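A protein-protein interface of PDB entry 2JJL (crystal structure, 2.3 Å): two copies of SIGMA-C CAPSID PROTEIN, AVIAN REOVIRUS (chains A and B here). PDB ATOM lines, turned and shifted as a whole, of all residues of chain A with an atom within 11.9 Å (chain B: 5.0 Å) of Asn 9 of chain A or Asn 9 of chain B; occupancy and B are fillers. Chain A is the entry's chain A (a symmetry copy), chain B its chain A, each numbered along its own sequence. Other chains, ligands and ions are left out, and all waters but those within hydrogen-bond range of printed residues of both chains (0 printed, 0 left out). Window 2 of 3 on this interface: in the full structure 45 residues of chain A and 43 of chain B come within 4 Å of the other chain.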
ATOM      1  N   THR A   5       3.920  19.645  10.759  1.00  0.00           N
ATOM      2  CA  THR A   5       2.565  20.089  10.324  1.00  0.00           C
ATOM      3  C   THR A   5       1.571  20.208  11.478  1.00  0.00           C
ATOM      4  O   THR A   5       0.796  21.156  11.526  1.00  0.00           O
ATOM      5  CB  THR A   5       1.954  19.184   9.261  1.00  0.00           C
ATOM      6  OG1 THR A   5       1.700  17.895   9.814  1.00  0.00           O
ATOM      7  CG2 THR A   5       2.861  19.079   8.049  1.00  0.00           C
ATOM      8  N   VAL A   6       1.594  19.250  12.402  1.00  0.00           N
ATOM      9  CA  VAL A   6       0.864  19.420  13.662  1.00  0.00           C
ATOM     10  C   VAL A   6       1.461  20.632  14.411  1.00  0.00           C
ATOM     11  O   VAL A   6       0.742  21.446  15.001  1.00  0.00           O
ATOM     12  CB  VAL A   6       0.968  18.164  14.560  1.00  0.00           C
ATOM     13  CG1 VAL A   6       0.428  18.463  15.957  1.00  0.00           C
ATOM     14  CG2 VAL A   6       0.262  16.977  13.921  1.00  0.00           C
ATOM     15  N   ASP A   7       2.787  20.709  14.392  1.00  0.00           N
ATOM     16  CA  ASP A   7       3.506  21.785  15.010  1.00  0.00           C
ATOM     17  C   ASP A   7       3.302  23.128  14.270  1.00  0.00           C
ATOM     18  O   ASP A   7       3.178  24.152  14.909  1.00  0.00           O
ATOM     19  CB  ASP A   7       4.979  21.451  15.071  1.00  0.00           C
ATOM     20  CG  ASP A   7       5.732  22.428  15.925  1.00  0.00           C
ATOM     21  OD1 ASP A   7       5.769  22.208  17.125  1.00  0.00           O
ATOM     22  OD2 ASP A   7       6.200  23.469  15.425  1.00  0.00           O
ATOM     23  N   GLY A   8       3.296  23.093  12.939  1.00  0.00           N
ATOM     24  CA  GLY A   8       2.954  24.232  12.079  1.00  0.00           C
ATOM     25  C   GLY A   8       1.541  24.763  12.299  1.00  0.00           C
ATOM     26  O   GLY A   8       1.373  25.960  12.492  1.00  0.00           O
ATOM     27  N   ASN A   9       0.541  23.869  12.296  1.00  0.00           N
ATOM     28  CA  ASN A   9      -0.840  24.219  12.647  1.00  0.00           C
ATOM     29  C   ASN A   9      -0.935  24.814  14.040  1.00  0.00           C
ATOM     30  O   ASN A   9      -1.678  25.774  14.257  1.00  0.00           O
ATOM     31  CB  ASN A   9      -1.785  23.021  12.527  1.00  0.00           C
ATOM     32  CG  ASN A   9      -2.079  22.657  11.089  1.00  0.00           C
ATOM     33  OD1 ASN A   9      -1.748  23.436  10.210  1.00  0.00           O
ATOM     34  ND2 ASN A   9      -2.692  21.455  10.833  1.00  0.00           N
ATOM     35  N   SER A  10      -0.165  24.280  14.988  1.00  0.00           N
ATOM     36  CA  SER A  10      -0.239  24.800  16.356  1.00  0.00           C
ATOM     37  C   SER A  10       0.320  26.226  16.460  1.00  0.00           C
ATOM     38  O   SER A  10      -0.217  27.063  17.187  1.00  0.00           O
ATOM     39  CB  SER A  10       0.451  23.868  17.326  1.00  0.00           C
ATOM     40  OG  SER A  10       0.570  24.494  18.598  1.00  0.00           O
ATOM     41  N   THR A  11       1.377  26.503  15.700  1.00  0.00           N
ATOM     42  CA  THR A  11       1.924  27.827  15.601  1.00  0.00           C
ATOM     43  C   THR A  11       0.926  28.804  14.931  1.00  0.00           C
ATOM     44  O   THR A  11       0.766  29.919  15.406  1.00  0.00           O
ATOM     45  CB  THR A  11       3.267  27.768  14.847  1.00  0.00           C
ATOM     46  OG1 THR A  11       4.202  27.061  15.660  1.00  0.00           O
ATOM     47  CG2 THR A  11       3.821  29.178  14.555  1.00  0.00           C
ATOM     48  N   ALA A  12       0.276  28.380  13.839  1.00  0.00           N
ATOM     49  CA  ALA A  12      -0.790  29.165  13.207  1.00  0.00           C
ATOM     50  C   ALA A  12      -1.941  29.468  14.192  1.00  0.00           C
ATOM     51  O   ALA A  12      -2.407  30.596  14.263  1.00  0.00           O
ATOM     52  CB  ALA A  12      -1.309  28.474  11.984  1.00  0.00           C
ATOM     53  N   ILE A  13      -2.368  28.461  14.951  1.00  0.00           N
ATOM     54  CA  ILE A  13      -3.411  28.609  15.960  1.00  0.00           C
ATOM     55  C   ILE A  13      -3.027  29.630  17.039  1.00  0.00           C
ATOM     56  O   ILE A  13      -3.869  30.408  17.462  1.00  0.00           O
ATOM     57  CB  ILE A  13      -3.792  27.239  16.606  1.00  0.00           C
ATOM     58  CG1 ILE A  13      -4.563  26.392  15.601  1.00  0.00           C
ATOM     59  CG2 ILE A  13      -4.540  27.428  17.964  1.00  0.00           C
ATOM     60  CD1 ILE A  13      -4.686  24.887  15.990  1.00  0.00           C
ATOM     61  N   SER A  14      -1.776  29.610  17.494  1.00  0.00           N
ATOM     62  CA  SER A  14      -1.295  30.581  18.478  1.00  0.00           C
ATOM     63  C   SER A  14      -1.321  32.003  17.915  1.00  0.00           C
ATOM     64  O   SER A  14      -1.720  32.915  18.607  1.00  0.00           O
ATOM     65  CB  SER A  14       0.128  30.243  18.949  1.00  0.00           C
ATOM     66  OG  SER A  14       0.113  29.067  19.747  1.00  0.00           O
ATOM     67  N   ASN A  15      -0.874  32.177  16.673  1.00  0.00           N
ATOM     68  CA  ASN A  15      -1.041  33.447  15.957  1.00  0.00           C
ATOM     69  C   ASN A  15      -2.489  33.934  15.834  1.00  0.00           C
ATOM     70  O   ASN A  15      -2.750  35.090  16.072  1.00  0.00           O
ATOM     71  CB  ASN A  15      -0.376  33.386  14.580  1.00  0.00           C
ATOM     72  CG  ASN A  15       1.131  33.196  14.678  1.00  0.00           C
ATOM     73  OD1 ASN A  15       1.730  33.443  15.730  1.00  0.00           O
ATOM     74  ND2 ASN A  15       1.750  32.732  13.585  1.00  0.00           N
ATOM     75  N   LEU A  16      -3.426  33.051  15.491  1.00  0.00           N
ATOM     76  CA  LEU A  16      -4.828  33.441  15.378  1.00  0.00           C
ATOM     77  C   LEU A  16      -5.356  33.911  16.733  1.00  0.00           C
ATOM     78  O   LEU A  16      -6.066  34.906  16.813  1.00  0.00           O
ATOM     79  CB  LEU A  16      -5.700  32.290  14.862  1.00  0.00           C
ATOM     80  CG  LEU A  16      -5.434  31.644  13.493  1.00  0.00           C
ATOM     81  CD1 LEU A  16      -6.515  30.639  13.203  1.00  0.00           C
ATOM     82  CD2 LEU A  16      -5.336  32.621  12.361  1.00  0.00           C
ATOM     83  N   LYS A  17      -5.003  33.182  17.783  1.00  0.00           N
ATOM     84  CA  LYS A  17      -5.435  33.453  19.139  1.00  0.00           C
ATOM     85  C   LYS A  17      -5.036  34.872  19.556  1.00  0.00           C
ATOM     86  O   LYS A  17      -5.824  35.597  20.166  1.00  0.00           O
ATOM     87  CB  LYS A  17      -4.764  32.445  20.054  1.00  0.00           C
ATOM     88  CG  LYS A  17      -5.248  32.398  21.490  1.00  0.00           C
ATOM     89  CD  LYS A  17      -4.473  31.314  22.274  1.00  0.00           C
ATOM     90  CE  LYS A  17      -4.636  29.918  21.643  1.00  0.00           C
ATOM     91  NZ  LYS A  17      -4.216  28.805  22.554  1.00  0.00           N
ATOM     92  N   SER A  18      -3.803  35.237  19.213  1.00  0.00           N
ATOM     93  CA  SER A  18      -3.253  36.555  19.446  1.00  0.00           C
ATOM     94  C   SER A  18      -4.063  37.653  18.727  1.00  0.00           C
ATOM     95  O   SER A  18      -4.416  38.650  19.345  1.00  0.00           O
ATOM     96  CB  SER A  18      -1.798  36.568  18.989  1.00  0.00           C
ATOM     97  OG  SER A  18      -1.183  37.792  19.314  1.00  0.00           O
ATOM     98  N   ILE A  20      -7.212  37.324  17.623  1.00  0.00           N
ATOM     99  CA  ILE A  20      -8.566  37.315  18.150  1.00  0.00           C
ATOM    100  C   ILE A  20      -8.597  38.181  19.409  1.00  0.00           C
ATOM    101  O   ILE A  20      -9.538  38.961  19.606  1.00  0.00           O
ATOM    102  CB  ILE A  20      -9.040  35.872  18.457  1.00  0.00           C
ATOM    103  CG1 ILE A  20      -9.332  35.104  17.153  1.00  0.00           C
ATOM    104  CG2 ILE A  20     -10.225  35.869  19.389  1.00  0.00           C
ATOM    105  CD1 ILE A  20      -9.461  33.563  17.349  1.00  0.00           C
ATOM    106  N   THR B   5      -6.660  15.042   8.195  1.00  0.00           N
ATOM    107  CA  THR B   5      -6.948  15.747   9.476  1.00  0.00           C
ATOM    108  C   THR B   5      -5.990  16.903   9.754  1.00  0.00           C
ATOM    109  O   THR B   5      -6.416  17.958  10.211  1.00  0.00           O
ATOM    110  CB  THR B   5      -6.936  14.817  10.684  1.00  0.00           C
ATOM    111  OG1 THR B   5      -5.619  14.314  10.890  1.00  0.00           O
ATOM    112  CG2 THR B   5      -7.924  13.680  10.504  1.00  0.00           C
ATOM    113  N   VAL B   6      -4.702  16.706   9.483  1.00  0.00           N
ATOM    114  CA  VAL B   6      -3.766  17.834   9.475  1.00  0.00           C
ATOM    115  C   VAL B   6      -4.201  18.820   8.369  1.00  0.00           C
ATOM    116  O   VAL B   6      -4.171  20.043   8.545  1.00  0.00           O
ATOM    117  CB  VAL B   6      -2.314  17.374   9.203  1.00  0.00           C
ATOM    118  CG1 VAL B   6      -1.414  18.579   8.942  1.00  0.00           C
ATOM    119  CG2 VAL B   6      -1.791  16.514  10.346  1.00  0.00           C
ATOM    120  N   ASP B   7      -4.577  18.257   7.227  1.00  0.00           N
ATOM    121  CA  ASP B   7      -5.041  19.021   6.105  1.00  0.00           C
ATOM    122  C   ASP B   7      -6.418  19.674   6.370  1.00  0.00           C
ATOM    123  O   ASP B   7      -6.636  20.799   5.972  1.00  0.00           O
ATOM    124  CB  ASP B   7      -5.117  18.140   4.878  1.00  0.00           C
ATOM    125  CG  ASP B   7      -5.357  18.945   3.635  1.00  0.00           C
ATOM    126  OD1 ASP B   7      -4.378  19.412   3.075  1.00  0.00           O
ATOM    127  OD2 ASP B   7      -6.520  19.203   3.268  1.00  0.00           O
ATOM    128  N   GLY B   8      -7.322  18.941   7.015  1.00  0.00           N
ATOM    129  CA  GLY B   8      -8.614  19.448   7.495  1.00  0.00           C
ATOM    130  C   GLY B   8      -8.489  20.592   8.499  1.00  0.00           C
ATOM    131  O   GLY B   8      -9.124  21.622   8.316  1.00  0.00           O
ATOM    132  N   ASN B   9      -7.653  20.413   9.531  1.00  0.00           N
ATOM    133  CA  ASN B   9      -7.321  21.483  10.479  1.00  0.00           C
ATOM    134  C   ASN B   9      -6.728  22.692   9.781  1.00  0.00           C
ATOM    135  O   ASN B   9      -7.051  23.832  10.126  1.00  0.00           O
ATOM    136  CB  ASN B   9      -6.374  21.001  11.581  1.00  0.00           C
ATOM    137  CG  ASN B   9      -7.063  20.110  12.589  1.00  0.00           C
ATOM    138  OD1 ASN B   9      -8.282  20.043  12.572  1.00  0.00           O
ATOM    139  ND2 ASN B   9      -6.286  19.401  13.473  1.00  0.00           N
ATOM    140  N   SER B  10      -5.884  22.466   8.774  1.00  0.00           N
ATOM    141  CA  SER B  10      -5.263  23.599   8.084  1.00  0.00           C
ATOM    142  C   SER B  10      -6.286  24.411   7.275  1.00  0.00           C
ATOM    143  O   SER B  10      -6.218  25.640   7.226  1.00  0.00           O
ATOM    144  CB  SER B  10      -4.117  23.139   7.212  1.00  0.00           C
ATOM    145  OG  SER B  10      -3.679  24.208   6.382  1.00  0.00           O
ATOM    146  N   THR B  11      -7.250  23.718   6.677  1.00  0.00           N
ATOM    147  CA  THR B  11      -8.343  24.355   5.997  1.00  0.00           C
ATOM    148  C   THR B  11      -9.238  25.148   6.980  1.00  0.00           C
ATOM    149  O   THR B  11      -9.623  26.268   6.672  1.00  0.00           O
ATOM    150  CB  THR B  11      -9.144  23.293   5.217  1.00  0.00           C
ATOM    151  OG1 THR B  11      -8.317  22.797   4.167  1.00  0.00           O
ATOM    152  CG2 THR B  11     -10.430  23.886   4.605  1.00  0.00           C
ATOM    153  N   ALA B  12      -9.562  24.563   8.140  1.00  0.00           N
ATOM    154  CA  ALA B  12     -10.285  25.272   9.202  1.00  0.00           C
ATOM    155  C   ALA B  12      -9.533  26.542   9.660  1.00  0.00           C
ATOM    156  O   ALA B  12     -10.137  27.594   9.804  1.00  0.00           O
ATOM    157  CB  ALA B  12     -10.552  24.367  10.365  1.00  0.00           C
ATOM    158  N   ILE B  13      -8.222  26.427   9.862  1.00  0.00           N
ATOM    159  CA  ILE B  13      -7.373  27.549  10.246  1.00  0.00           C
ATOM    160  C   ILE B  13      -7.399  28.674   9.203  1.00  0.00           C
ATOM    161  O   ILE B  13      -7.432  29.839   9.571  1.00  0.00           O
ATOM    162  CB  ILE B  13      -5.906  27.096  10.532  1.00  0.00           C
ATOM    163  CG1 ILE B  13      -5.855  26.312  11.838  1.00  0.00           C
ATOM    164  CG2 ILE B  13      -4.910  28.298  10.491  1.00  0.00           C
ATOM    165  CD1 ILE B  13      -4.536  25.506  12.053  1.00  0.00           C
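Among the printed residues, pairs that only touch across the chains: Thr 5 of chain A with Val 6 of chain B (3.3 Å), Asn 9 of chain A with Ile 13 of chain B (3.6 Å), Ile 13 of chain A with Ile 13 of chain B (3.7 Å), Asn 9 of chain A with Asn 9 of chain B (3.8 Å), Leu 16 of chain A with Ile 13 of chain B (3.8 Å), Asn 9 of chain A with Ser 10 of chain B (3.8 Å) and Ala 12 of chain A with Ile 13 of chain B (3.9 Å).
Hydrophobic or aromatic side chains of chain A that line the printed part of chain B: Ala 12, Ile 13 and Leu 16.
Among the printed residues, no Asp or Glu carboxylate lies within 4 Å of a Lys or Arg side-chain nitrogen of the other chain.
Printed residues of chain B within 4 Å of Asn 9 of chain A: Val 6 (3.1 Å), Asn 9 (3.8 Å), Ser 10 (3.8 Å) and Ile 13 (3.6 Å).
Printed residues of chain A within 4 Å of Asn 9 of chain B: Asn 9.
Val 6 of chain B touches just these residues of chain A: Thr 5 (3.3 Å) and Asn 9 (3.1 Å).
No residue of chain A comes within 4 Å of Gly 8 of chain B.
Of chain A, only Asn 9 (3.8 Å) comes within 4 Å of Ser 10 of chain B.
Thr 11 of chain B touches none of the printed residues of chain A.
No residue of chain A comes within 4 Å of Ala 12 of chain B.
Ile 13 of chain B touches just these residues of chain A: Asn 9 (3.6 Å), Ala 12 (3.9 Å), Ile 13 (3.7 Å) and Leu 16 (3.8 Å).
Printed residues of chain B within 4 Å of Ala 12 of chain A: Ile 13.
Of the printed residues of chain B, Ile 13 of chain A touches Ile 13.
Printed residues of chain B within 4 Å of Thr 5 of chain A: Val 6.
Printed residues of chain B within 4 Å of Leu 16 of chain A: Ile 13.
Gly 8 of chain A touches none of the printed residues of chain B.
Ser 10 of chain A touches none of the printed residues of chain B.
The nearest printed residue of chain B that does not touch Asn 9 of chain A is Thr 5 of chain B (5.1 Å).
Thr 5 of chain A touches Val 6 of chain B, but with the chains exchanged Val 6 of chain A does not touch Thr 5 of chain B (7.1 Å).
Asn 9 of chain A touches Val 6 of chain B, but with the chains exchanged Val 6 of chain A does not touch Asn 9 of chain B (7.0 Å).
Asn 9 of chain A touches Ser 10 of chain B, but with the chains exchanged Ser 10 of chain A does not touch Asn 9 of chain B (7.8 Å).
Asn 9 of chain A touches Ile 13 of chain B, but with the chains exchanged Ile 13 of chain A does not touch Asn 9 of chain B (6.1 Å).
The backbone carbonyl oxygen of Val 6 of chain B lies within hydrogen-bond range of the side-chain amide nitrogen of Asn 9 of chain A (3.1 Å).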
